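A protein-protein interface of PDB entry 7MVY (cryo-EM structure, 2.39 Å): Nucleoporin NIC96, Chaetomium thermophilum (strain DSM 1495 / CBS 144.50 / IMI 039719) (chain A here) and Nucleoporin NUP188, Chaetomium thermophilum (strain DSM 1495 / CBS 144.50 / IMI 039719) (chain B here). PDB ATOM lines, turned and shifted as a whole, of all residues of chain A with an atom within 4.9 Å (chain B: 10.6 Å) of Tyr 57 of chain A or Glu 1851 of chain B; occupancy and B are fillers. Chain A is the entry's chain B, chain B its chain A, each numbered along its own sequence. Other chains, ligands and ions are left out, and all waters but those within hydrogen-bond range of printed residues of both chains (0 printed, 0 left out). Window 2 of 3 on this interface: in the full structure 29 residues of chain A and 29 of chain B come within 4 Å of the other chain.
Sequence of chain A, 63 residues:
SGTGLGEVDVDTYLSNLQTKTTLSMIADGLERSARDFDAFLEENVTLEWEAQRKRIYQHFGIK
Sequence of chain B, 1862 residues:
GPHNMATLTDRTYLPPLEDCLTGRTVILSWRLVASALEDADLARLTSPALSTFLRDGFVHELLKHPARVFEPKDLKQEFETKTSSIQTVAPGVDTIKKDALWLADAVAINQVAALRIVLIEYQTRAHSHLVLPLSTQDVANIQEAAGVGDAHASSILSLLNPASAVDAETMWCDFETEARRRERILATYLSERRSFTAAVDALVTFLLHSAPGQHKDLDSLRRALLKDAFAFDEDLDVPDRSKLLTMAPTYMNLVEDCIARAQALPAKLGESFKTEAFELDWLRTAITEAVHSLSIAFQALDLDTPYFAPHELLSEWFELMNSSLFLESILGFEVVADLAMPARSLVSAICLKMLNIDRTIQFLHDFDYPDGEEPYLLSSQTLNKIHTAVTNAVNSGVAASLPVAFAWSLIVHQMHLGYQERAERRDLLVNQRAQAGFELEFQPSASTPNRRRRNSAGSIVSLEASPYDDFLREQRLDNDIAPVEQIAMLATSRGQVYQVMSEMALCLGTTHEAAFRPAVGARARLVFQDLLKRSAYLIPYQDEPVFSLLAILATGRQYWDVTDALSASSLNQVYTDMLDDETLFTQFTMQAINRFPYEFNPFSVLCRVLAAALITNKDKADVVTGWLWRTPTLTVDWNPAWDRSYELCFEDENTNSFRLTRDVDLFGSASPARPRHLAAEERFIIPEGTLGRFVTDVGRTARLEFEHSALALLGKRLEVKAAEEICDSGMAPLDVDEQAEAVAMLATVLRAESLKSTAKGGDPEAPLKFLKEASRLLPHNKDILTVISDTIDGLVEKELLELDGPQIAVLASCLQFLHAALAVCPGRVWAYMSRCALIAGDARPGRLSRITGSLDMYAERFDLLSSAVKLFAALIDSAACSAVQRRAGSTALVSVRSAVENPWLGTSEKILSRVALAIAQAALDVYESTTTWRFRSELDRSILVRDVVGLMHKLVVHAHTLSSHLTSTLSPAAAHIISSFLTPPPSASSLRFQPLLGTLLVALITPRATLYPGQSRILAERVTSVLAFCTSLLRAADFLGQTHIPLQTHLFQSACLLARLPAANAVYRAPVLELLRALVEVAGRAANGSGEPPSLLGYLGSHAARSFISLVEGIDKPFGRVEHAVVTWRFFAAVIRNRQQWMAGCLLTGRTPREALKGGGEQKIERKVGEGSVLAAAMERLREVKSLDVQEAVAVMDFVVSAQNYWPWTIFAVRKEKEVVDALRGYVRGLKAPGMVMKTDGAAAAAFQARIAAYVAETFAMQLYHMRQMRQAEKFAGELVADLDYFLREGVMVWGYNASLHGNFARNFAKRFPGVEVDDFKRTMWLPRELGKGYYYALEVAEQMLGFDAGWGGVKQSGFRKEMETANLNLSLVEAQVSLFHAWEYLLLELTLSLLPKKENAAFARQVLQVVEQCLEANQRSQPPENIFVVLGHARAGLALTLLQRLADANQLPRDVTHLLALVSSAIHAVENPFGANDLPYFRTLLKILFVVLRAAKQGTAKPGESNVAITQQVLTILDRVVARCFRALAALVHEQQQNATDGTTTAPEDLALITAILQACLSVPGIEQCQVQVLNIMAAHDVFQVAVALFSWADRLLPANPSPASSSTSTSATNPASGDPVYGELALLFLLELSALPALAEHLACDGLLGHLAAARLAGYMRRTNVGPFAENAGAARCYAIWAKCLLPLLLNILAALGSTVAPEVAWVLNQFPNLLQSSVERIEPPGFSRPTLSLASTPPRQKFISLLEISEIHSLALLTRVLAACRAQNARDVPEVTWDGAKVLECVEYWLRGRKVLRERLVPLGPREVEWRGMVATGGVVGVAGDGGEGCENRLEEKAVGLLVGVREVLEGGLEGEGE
ND1 of His 1756 of chain B sits close to NH1 of Arg 53 of chain A.
Leu 1845 of chain B touches Arg 53 of chain A (CG to NH2, 3.4 Å).
OH of Tyr 57 of chain A touches CG of Glu 1851 of chain B, at 3.4 Å.
CZ of Phe 60 of chain A touches CB of Ala 1697 of chain B, at 3.5 Å.
Of the printed residues of chain B, Arg 53 of chain A touches His 1756 and Leu 1845.
No residue of chain B comes within 4 Å of Ile 56 of chain A.
Of chain B, only Glu 1851 (3.4 Å) comes within 4 Å of Tyr 57 of chain A.
No residue of chain B comes within 4 Å of Gln 58 of chain A.
Phe 60 of chain A touches just one residue of chain B: Ala 1697.
No residue of chain B comes within 4 Å of Gly 61 of chain A.
Printed residues of chain A within 4 Å of Ala 1697 of chain B: Phe 60 (3.5 Å).
Printed residues of chain A within 4 Å of His 1756 of chain B: Arg 53 (3.1 Å).
Leu 1787 of chain B touches none of the printed residues of chain A.
Of the printed residues of chain A, Leu 1845 of chain B touches Arg 53 (3.4 Å).
Printed residues of chain A within 4 Å of Glu 1851 of chain B: Tyr 57 (3.4 Å).
The nearest residue of chain B that does not touch Tyr 57 of chain A is Val 1852 of chain B (5.0 Å).
The nearest printed residue of chain A that does not touch Ala 1697 of chain B is Ile 56 of chain A (4.8 Å).
Hydrophobic or aromatic side chains of chain A that line the printed part of chain B: Tyr 57 and Phe 60.
Of the 22 printed residues of chain B, 4 touch a printed residue of chain A.
Printed residues of chain B that touch a printed residue of chain A: Ala 1697, His 1756, Leu 1845 and Glu 1851.
Hydrophobic or aromatic side chains of chain B that line the printed part of chain A: Ala 1697, His 1756 and Leu 1845.
Among the printed residues, 4 pairs touch across the chains.
Among the printed residues, no Asp or Glu carboxylate lies within 4 Å of a Lys or Arg side-chain nitrogen of the other chain.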
ATOM      1  N   ARG A  53      16.082 -17.487  21.379  1.00  0.00           N
ATOM      2  CA  ARG A  53      14.735 -17.887  20.985  1.00  0.00           C
ATOM      3  C   ARG A  53      14.695 -18.301  19.520  1.00  0.00           C
ATOM      4  O   ARG A  53      14.016 -19.269  19.157  1.00  0.00           O
ATOM      5  CB  ARG A  53      13.754 -16.747  21.251  1.00  0.00           C
ATOM      6  CG  ARG A  53      12.402 -16.922  20.583  1.00  0.00           C
ATOM      7  CD  ARG A  53      11.383 -15.942  21.135  1.00  0.00           C
ATOM      8  NE  ARG A  53      10.190 -15.864  20.300  1.00  0.00           N
ATOM      9  CZ  ARG A  53       9.081 -15.214  20.637  1.00  0.00           C
ATOM     10  NH1 ARG A  53       8.047 -15.196  19.807  1.00  0.00           N
ATOM     11  NH2 ARG A  53       9.001 -14.586  21.803  1.00  0.00           N
ATOM     12  N   LYS A  54      15.425 -17.585  18.661  1.00  0.00           N
ATOM     13  CA  LYS A  54      15.440 -17.926  17.243  1.00  0.00           C
ATOM     14  C   LYS A  54      16.069 -19.295  17.011  1.00  0.00           C
ATOM     15  O   LYS A  54      15.553 -20.097  16.224  1.00  0.00           O
ATOM     16  CB  LYS A  54      16.190 -16.850  16.456  1.00  0.00           C
ATOM     17  CG  LYS A  54      16.176 -17.045  14.945  1.00  0.00           C
ATOM     18  CD  LYS A  54      14.771 -16.930  14.375  1.00  0.00           C
ATOM     19  CE  LYS A  54      14.777 -17.031  12.859  1.00  0.00           C
ATOM     20  NZ  LYS A  54      13.408 -16.904  12.284  1.00  0.00           N
ATOM     21  N   ARG A  55      17.184 -19.583  17.688  1.00  0.00           N
ATOM     22  CA  ARG A  55      17.824 -20.883  17.514  1.00  0.00           C
ATOM     23  C   ARG A  55      16.951 -21.997  18.077  1.00  0.00           C
ATOM     24  O   ARG A  55      16.890 -23.092  17.507  1.00  0.00           O
ATOM     25  CB  ARG A  55      19.210 -20.887  18.165  1.00  0.00           C
ATOM     26  CG  ARG A  55      19.241 -21.313  19.628  1.00  0.00           C
ATOM     27  CD  ARG A  55      20.639 -21.192  20.213  1.00  0.00           C
ATOM     28  NE  ARG A  55      21.123 -19.815  20.206  1.00  0.00           N
ATOM     29  CZ  ARG A  55      22.308 -19.433  20.672  1.00  0.00           C
ATOM     30  NH1 ARG A  55      23.143 -20.325  21.189  1.00  0.00           N
ATOM     31  NH2 ARG A  55      22.661 -18.156  20.623  1.00  0.00           N
ATOM     32  N   ILE A  56      16.252 -21.736  19.184  1.00  0.00           N
ATOM     33  CA  ILE A  56      15.341 -22.737  19.729  1.00  0.00           C
ATOM     34  C   ILE A  56      14.201 -23.008  18.754  1.00  0.00           C
ATOM     35  O   ILE A  56      13.795 -24.159  18.554  1.00  0.00           O
ATOM     36  CB  ILE A  56      14.816 -22.285  21.105  1.00  0.00           C
ATOM     37  CG1 ILE A  56      15.954 -22.285  22.130  1.00  0.00           C
ATOM     38  CG2 ILE A  56      13.681 -23.191  21.562  1.00  0.00           C
ATOM     39  CD1 ILE A  56      15.609 -21.597  23.436  1.00  0.00           C
ATOM     40  N   TYR A  57      13.671 -21.954  18.128  1.00  0.00           N
ATOM     41  CA  TYR A  57      12.606 -22.137  17.146  1.00  0.00           C
ATOM     42  C   TYR A  57      13.103 -22.921  15.938  1.00  0.00           C
ATOM     43  O   TYR A  57      12.400 -23.800  15.426  1.00  0.00           O
ATOM     44  CB  TYR A  57      12.055 -20.778  16.714  1.00  0.00           C
ATOM     45  CG  TYR A  57      11.134 -20.842  15.517  1.00  0.00           C
ATOM     46  CD1 TYR A  57       9.790 -21.160  15.666  1.00  0.00           C
ATOM     47  CD2 TYR A  57      11.607 -20.582  14.238  1.00  0.00           C
ATOM     48  CE1 TYR A  57       8.944 -21.218  14.574  1.00  0.00           C
ATOM     49  CE2 TYR A  57      10.770 -20.639  13.141  1.00  0.00           C
ATOM     50  CZ  TYR A  57       9.439 -20.957  13.314  1.00  0.00           C
ATOM     51  OH  TYR A  57       8.602 -21.013  12.224  1.00  0.00           O
ATOM     52  N   GLN A  58      14.315 -22.616  15.467  1.00  0.00           N
ATOM     53  CA  GLN A  58      14.870 -23.354  14.338  1.00  0.00           C
ATOM     54  C   GLN A  58      15.138 -24.809  14.700  1.00  0.00           C
ATOM     55  O   GLN A  58      15.043 -25.689  13.837  1.00  0.00           O
ATOM     56  CB  GLN A  58      16.155 -22.684  13.851  1.00  0.00           C
ATOM     57  CG  GLN A  58      15.948 -21.305  13.235  1.00  0.00           C
ATOM     58  CD  GLN A  58      15.022 -21.321  12.029  1.00  0.00           C
ATOM     59  OE1 GLN A  58      14.230 -20.400  11.832  1.00  0.00           O
ATOM     60  NE2 GLN A  58      15.123 -22.365  11.212  1.00  0.00           N
ATOM     61  N   HIS A  59      15.474 -25.081  15.963  1.00  0.00           N
ATOM     62  CA  HIS A  59      15.676 -26.461  16.391  1.00  0.00           C
ATOM     63  C   HIS A  59      14.354 -27.214  16.460  1.00  0.00           C
ATOM     64  O   HIS A  59      14.269 -28.369  16.029  1.00  0.00           O
ATOM     65  CB  HIS A  59      16.382 -26.489  17.747  1.00  0.00           C
ATOM     66  CG  HIS A  59      16.610 -27.869  18.279  1.00  0.00           C
ATOM     67  ND1 HIS A  59      15.689 -28.525  19.068  1.00  0.00           N
ATOM     68  CD2 HIS A  59      17.656 -28.718  18.137  1.00  0.00           C
ATOM     69  CE1 HIS A  59      16.156 -29.719  19.388  1.00  0.00           C
ATOM     70  NE2 HIS A  59      17.348 -29.860  18.836  1.00  0.00           N
ATOM     71  N   PHE A  60      13.312 -26.578  17.001  1.00  0.00           N
ATOM     72  CA  PHE A  60      12.001 -27.218  17.041  1.00  0.00           C
ATOM     73  C   PHE A  60      11.472 -27.464  15.633  1.00  0.00           C
ATOM     74  O   PHE A  60      11.022 -28.570  15.310  1.00  0.00           O
ATOM     75  CB  PHE A  60      11.017 -26.359  17.840  1.00  0.00           C
ATOM     76  CG  PHE A  60      11.352 -26.235  19.305  1.00  0.00           C
ATOM     77  CD1 PHE A  60      12.259 -27.091  19.912  1.00  0.00           C
ATOM     78  CD2 PHE A  60      10.743 -25.260  20.079  1.00  0.00           C
ATOM     79  CE1 PHE A  60      12.555 -26.969  21.257  1.00  0.00           C
ATOM     80  CE2 PHE A  60      11.035 -25.136  21.423  1.00  0.00           C
ATOM     81  CZ  PHE A  60      11.943 -25.992  22.012  1.00  0.00           C
ATOM     82  N   GLY A  61      11.516 -26.443  14.783  1.00  0.00           N
ATOM     83  CA  GLY A  61      11.042 -26.568  13.417  1.00  0.00           C
ATOM     84  C   GLY A  61       9.532 -26.653  13.326  1.00  0.00           C
ATOM     85  O   GLY A  61       8.826 -26.394  14.301  1.00  0.00           O
ATOM     86  N   LEU B1693      10.672 -22.110  29.373  1.00  0.00           N
ATOM     87  CA  LEU B1693      10.798 -22.563  27.990  1.00  0.00           C
ATOM     88  C   LEU B1693      12.065 -23.387  27.796  1.00  0.00           C
ATOM     89  O   LEU B1693      12.052 -24.404  27.092  1.00  0.00           O
ATOM     90  CB  LEU B1693      10.791 -21.365  27.041  1.00  0.00           C
ATOM     91  CG  LEU B1693       9.483 -20.578  26.940  1.00  0.00           C
ATOM     92  CD1 LEU B1693       9.663 -19.372  26.031  1.00  0.00           C
ATOM     93  CD2 LEU B1693       8.353 -21.464  26.438  1.00  0.00           C
ATOM     94  N   ASN B1694      13.169 -22.963  28.412  1.00  0.00           N
ATOM     95  CA  ASN B1694      14.426 -23.689  28.262  1.00  0.00           C
ATOM     96  C   ASN B1694      14.330 -25.083  28.868  1.00  0.00           C
ATOM     97  O   ASN B1694      14.696 -26.077  28.229  1.00  0.00           O
ATOM     98  CB  ASN B1694      15.565 -22.898  28.907  1.00  0.00           C
ATOM     99  CG  ASN B1694      16.901 -23.605  28.795  1.00  0.00           C
ATOM    100  OD1 ASN B1694      17.268 -24.404  29.657  1.00  0.00           O
ATOM    101  ND2 ASN B1694      17.638 -23.312  27.730  1.00  0.00           N
ATOM    102  N   ALA B1697      12.246 -27.265  26.631  1.00  0.00           N
ATOM    103  CA  ALA B1697      12.859 -27.694  25.378  1.00  0.00           C
ATOM    104  C   ALA B1697      13.574 -29.030  25.543  1.00  0.00           C
ATOM    105  O   ALA B1697      13.535 -29.878  24.643  1.00  0.00           O
ATOM    106  CB  ALA B1697      13.830 -26.626  24.878  1.00  0.00           C
ATOM    107  N   HIS B1756       3.617 -15.539  23.864  1.00  0.00           N
ATOM    108  CA  HIS B1756       4.200 -16.559  22.999  1.00  0.00           C
ATOM    109  C   HIS B1756       4.599 -17.796  23.797  1.00  0.00           C
ATOM    110  O   HIS B1756       4.407 -18.929  23.339  1.00  0.00           O
ATOM    111  CB  HIS B1756       5.410 -15.994  22.258  1.00  0.00           C
ATOM    112  CG  HIS B1756       6.097 -16.990  21.378  1.00  0.00           C
ATOM    113  ND1 HIS B1756       5.623 -17.332  20.129  1.00  0.00           N
ATOM    114  CD2 HIS B1756       7.218 -17.725  21.568  1.00  0.00           C
ATOM    115  CE1 HIS B1756       6.425 -18.230  19.586  1.00  0.00           C
ATOM    116  NE2 HIS B1756       7.401 -18.487  20.438  1.00  0.00           N
ATOM    117  N   ALA B1759       1.493 -19.713  24.565  1.00  0.00           N
ATOM    118  CA  ALA B1759       1.008 -20.390  23.366  1.00  0.00           C
ATOM    119  C   ALA B1759       1.820 -21.648  23.085  1.00  0.00           C
ATOM    120  O   ALA B1759       1.261 -22.708  22.776  1.00  0.00           O
ATOM    121  CB  ALA B1759       1.060 -19.435  22.172  1.00  0.00           C
ATOM    122  N   LEU B1760       3.146 -21.548  23.188  1.00  0.00           N
ATOM    123  CA  LEU B1760       3.995 -22.711  22.953  1.00  0.00           C
ATOM    124  C   LEU B1760       3.737 -23.794  23.993  1.00  0.00           C
ATOM    125  O   LEU B1760       3.688 -24.987  23.664  1.00  0.00           O
ATOM    126  CB  LEU B1760       5.466 -22.291  22.958  1.00  0.00           C
ATOM    127  CG  LEU B1760       6.503 -23.320  22.495  1.00  0.00           C
ATOM    128  CD1 LEU B1760       7.783 -22.615  22.070  1.00  0.00           C
ATOM    129  CD2 LEU B1760       6.804 -24.347  23.578  1.00  0.00           C
ATOM    130  N   ARG B1763       0.516 -25.508  23.109  1.00  0.00           N
ATOM    131  CA  ARG B1763       0.692 -26.387  21.957  1.00  0.00           C
ATOM    132  C   ARG B1763       1.376 -27.688  22.362  1.00  0.00           C
ATOM    133  O   ARG B1763       0.927 -28.781  21.993  1.00  0.00           O
ATOM    134  CB  ARG B1763       1.496 -25.668  20.872  1.00  0.00           C
ATOM    135  CG  ARG B1763       1.697 -26.472  19.593  1.00  0.00           C
ATOM    136  CD  ARG B1763       0.377 -26.767  18.897  1.00  0.00           C
ATOM    137  NE  ARG B1763       0.572 -27.448  17.618  1.00  0.00           N
ATOM    138  CZ  ARG B1763       0.718 -28.763  17.479  1.00  0.00           C
ATOM    139  NH1 ARG B1763       0.698 -29.560  18.539  1.00  0.00           N
ATOM    140  NH2 ARG B1763       0.889 -29.284  16.272  1.00  0.00           N
ATOM    141  N   LEU B1787      -6.959 -14.566  21.703  1.00  0.00           N
ATOM    142  CA  LEU B1787      -7.150 -14.348  20.272  1.00  0.00           C
ATOM    143  C   LEU B1787      -7.725 -12.961  20.006  1.00  0.00           C
ATOM    144  O   LEU B1787      -7.233 -12.227  19.141  1.00  0.00           O
ATOM    145  CB  LEU B1787      -8.060 -15.431  19.693  1.00  0.00           C
ATOM    146  CG  LEU B1787      -7.439 -16.821  19.535  1.00  0.00           C
ATOM    147  CD1 LEU B1787      -8.502 -17.840  19.155  1.00  0.00           C
ATOM    148  CD2 LEU B1787      -6.322 -16.804  18.501  1.00  0.00           C
ATOM    149  N   VAL B1790      -4.867 -10.338  20.655  1.00  0.00           N
ATOM    150  CA  VAL B1790      -3.895 -10.245  19.572  1.00  0.00           C
ATOM    151  C   VAL B1790      -4.536  -9.721  18.295  1.00  0.00           C
ATOM    152  O   VAL B1790      -3.838  -9.174  17.434  1.00  0.00           O
ATOM    153  CB  VAL B1790      -3.219 -11.612  19.325  1.00  0.00           C
ATOM    154  CG1 VAL B1790      -2.496 -12.083  20.578  1.00  0.00           C
ATOM    155  CG2 VAL B1790      -4.237 -12.644  18.865  1.00  0.00           C
ATOM    156  N   LEU B1794      -3.249  -5.485  16.416  1.00  0.00           N
ATOM    157  CA  LEU B1794      -2.539  -5.752  15.170  1.00  0.00           C
ATOM    158  C   LEU B1794      -3.292  -5.156  13.986  1.00  0.00           C
ATOM    159  O   LEU B1794      -2.701  -4.856  12.949  1.00  0.00           O
ATOM    160  CB  LEU B1794      -2.351  -7.259  14.973  1.00  0.00           C
ATOM    161  CG  LEU B1794      -1.686  -7.693  13.664  1.00  0.00           C
ATOM    162  CD1 LEU B1794      -0.319  -7.047  13.505  1.00  0.00           C
ATOM    163  CD2 LEU B1794      -1.574  -9.209  13.604  1.00  0.00           C
ATOM    164  N   VAL B1843       6.178  -7.172  16.124  1.00  0.00           N
ATOM    165  CA  VAL B1843       5.633  -7.837  14.944  1.00  0.00           C
ATOM    166  C   VAL B1843       6.271  -9.208  14.760  1.00  0.00           C
ATOM    167  O   VAL B1843       5.605 -10.154  14.325  1.00  0.00           O
ATOM    168  CB  VAL B1843       5.804  -6.955  13.692  1.00  0.00           C
ATOM    169  CG1 VAL B1843       7.272  -6.690  13.400  1.00  0.00           C
ATOM    170  CG2 VAL B1843       5.126  -7.602  12.490  1.00  0.00           C
ATOM    171  N   GLY B1844       7.556  -9.351  15.094  1.00  0.00           N
ATOM    172  CA  GLY B1844       8.178 -10.663  15.021  1.00  0.00           C
ATOM    173  C   GLY B1844       7.548 -11.653  15.981  1.00  0.00           C
ATOM    174  O   GLY B1844       7.286 -12.804  15.622  1.00  0.00           O
ATOM    175  N   LEU B1845       7.289 -11.218  17.216  1.00  0.00           N
ATOM    176  CA  LEU B1845       6.637 -12.091  18.185  1.00  0.00           C
ATOM    177  C   LEU B1845       5.216 -12.429  17.753  1.00  0.00           C
ATOM    178  O   LEU B1845       4.749 -13.553  17.963  1.00  0.00           O
ATOM    179  CB  LEU B1845       6.636 -11.435  19.566  1.00  0.00           C
ATOM    180  CG  LEU B1845       7.853 -11.720  20.452  1.00  0.00           C
ATOM    181  CD1 LEU B1845       9.129 -11.115  19.885  1.00  0.00           C
ATOM    182  CD2 LEU B1845       7.607 -11.216  21.865  1.00  0.00           C
ATOM    183  N   LEU B1846       4.511 -11.472  17.145  1.00  0.00           N
ATOM    184  CA  LEU B1846       3.169 -11.759  16.647  1.00  0.00           C
ATOM    185  C   LEU B1846       3.209 -12.783  15.520  1.00  0.00           C
ATOM    186  O   LEU B1846       2.364 -13.686  15.461  1.00  0.00           O
ATOM    187  CB  LEU B1846       2.495 -10.469  16.178  1.00  0.00           C
ATOM    188  CG  LEU B1846       2.127  -9.464  17.272  1.00  0.00           C
ATOM    189  CD1 LEU B1846       1.585  -8.184  16.659  1.00  0.00           C
ATOM    190  CD2 LEU B1846       1.117 -10.060  18.242  1.00  0.00           C
ATOM    191  N   VAL B1847       4.183 -12.663  14.615  1.00  0.00           N
ATOM    192  CA  VAL B1847       4.329 -13.649  13.548  1.00  0.00           C
ATOM    193  C   VAL B1847       4.642 -15.019  14.135  1.00  0.00           C
ATOM    194  O   VAL B1847       4.119 -16.042  13.679  1.00  0.00           O
ATOM    195  CB  VAL B1847       5.412 -13.201  12.549  1.00  0.00           C
ATOM    196  CG1 VAL B1847       5.743 -14.326  11.579  1.00  0.00           C
ATOM    197  CG2 VAL B1847       4.953 -11.963  11.790  1.00  0.00           C
ATOM    198  N   GLY B1848       5.501 -15.062  15.156  1.00  0.00           N
ATOM    199  CA  GLY B1848       5.789 -16.331  15.807  1.00  0.00           C
ATOM    200  C   GLY B1848       4.559 -16.949  16.446  1.00  0.00           C
ATOM    201  O   GLY B1848       4.329 -18.156  16.339  1.00  0.00           O
ATOM    202  N   VAL B1849       3.754 -16.128  17.123  1.00  0.00           N
ATOM    203  CA  VAL B1849       2.523 -16.622  17.735  1.00  0.00           C
ATOM    204  C   VAL B1849       1.589 -17.174  16.666  1.00  0.00           C
ATOM    205  O   VAL B1849       0.994 -18.246  16.826  1.00  0.00           O
ATOM    206  CB  VAL B1849       1.848 -15.508  18.556  1.00  0.00           C
ATOM    207  CG1 VAL B1849       0.454 -15.937  18.992  1.00  0.00           C
ATOM    208  CG2 VAL B1849       2.697 -15.155  19.767  1.00  0.00           C
ATOM    209  N   ARG B1850       1.442 -16.444  15.557  1.00  0.00           N
ATOM    210  CA  ARG B1850       0.611 -16.930  14.461  1.00  0.00           C
ATOM    211  C   ARG B1850       1.143 -18.239  13.894  1.00  0.00           C
ATOM    212  O   ARG B1850       0.359 -19.102  13.482  1.00  0.00           O
ATOM    213  CB  ARG B1850       0.525 -15.874  13.358  1.00  0.00           C
ATOM    214  CG  ARG B1850      -0.262 -14.628  13.738  1.00  0.00           C
ATOM    215  CD  ARG B1850      -1.740 -14.936  13.930  1.00  0.00           C
ATOM    216  NE  ARG B1850      -2.537 -13.722  14.096  1.00  0.00           N
ATOM    217  CZ  ARG B1850      -3.015 -12.991  13.093  1.00  0.00           C
ATOM    218  NH1 ARG B1850      -2.782 -13.340  11.834  1.00  0.00           N
ATOM    219  NH2 ARG B1850      -3.730 -11.905  13.350  1.00  0.00           N
ATOM    220  N   GLU B1851       2.466 -18.406  13.864  1.00  0.00           N
ATOM    221  CA  GLU B1851       3.051 -19.626  13.320  1.00  0.00           C
ATOM    222  C   GLU B1851       2.869 -20.815  14.254  1.00  0.00           C
ATOM    223  O   GLU B1851       2.672 -21.942  13.783  1.00  0.00           O
ATOM    224  CB  GLU B1851       4.539 -19.408  13.034  1.00  0.00           C
ATOM    225  CG  GLU B1851       5.248 -20.610  12.420  1.00  0.00           C
ATOM    226  CD  GLU B1851       4.698 -20.987  11.058  1.00  0.00           C
ATOM    227  OE1 GLU B1851       3.940 -20.183  10.476  1.00  0.00           O
ATOM    228  OE2 GLU B1851       5.023 -22.090  10.570  1.00  0.00           O
ATOM    229  N   VAL B1852       2.928 -20.594  15.565  1.00  0.00           N
ATOM    230  CA  VAL B1852       2.764 -21.696  16.509  1.00  0.00           C
ATOM    231  C   VAL B1852       1.291 -21.997  16.779  1.00  0.00           C
ATOM    232  O   VAL B1852       0.934 -23.155  17.019  1.00  0.00           O
ATOM    233  CB  VAL B1852       3.510 -21.400  17.823  1.00  0.00           C
ATOM    234  CG1 VAL B1852       4.990 -21.159  17.555  1.00  0.00           C
ATOM    235  CG2 VAL B1852       2.887 -20.215  18.545  1.00  0.00           C
ATOM    236  N   LEU B1853       0.426 -20.983  16.748  1.00  0.00           N
ATOM    237  CA  LEU B1853      -1.000 -21.177  16.979  1.00  0.00           C
ATOM    238  C   LEU B1853      -1.800 -21.347  15.697  1.00  0.00           C
ATOM    239  O   LEU B1853      -2.848 -22.000  15.719  1.00  0.00           O
ATOM    240  CB  LEU B1853      -1.577 -19.995  17.768  1.00  0.00           C
ATOM    241  CG  LEU B1853      -1.091 -19.830  19.210  1.00  0.00           C
ATOM    242  CD1 LEU B1853      -1.722 -18.602  19.845  1.00  0.00           C
ATOM    243  CD2 LEU B1853      -1.398 -21.074  20.031  1.00  0.00           C
ATOM    244  N   GLU B1854      -1.336 -20.780  14.586  1.00  0.00           N
ATOM    245  CA  GLU B1854      -2.044 -20.886  13.315  1.00  0.00           C
ATOM    246  C   GLU B1854      -1.099 -21.343  12.209  1.00  0.00           C
ATOM    247  O   GLU B1854      -0.205 -22.156  12.439  1.00  0.00           O
ATOM    248  CB  GLU B1854      -2.682 -19.546  12.943  1.00  0.00           C
ATOM    249  CG  GLU B1854      -3.656 -19.008  13.981  1.00  0.00           C
ATOM    250  CD  GLU B1854      -4.881 -19.886  14.147  1.00  0.00           C
ATOM    251  OE1 GLU B1854      -5.070 -20.808  13.326  1.00  0.00           O
ATOM    252  OE2 GLU B1854      -5.655 -19.654  15.099  1.00  0.00           O
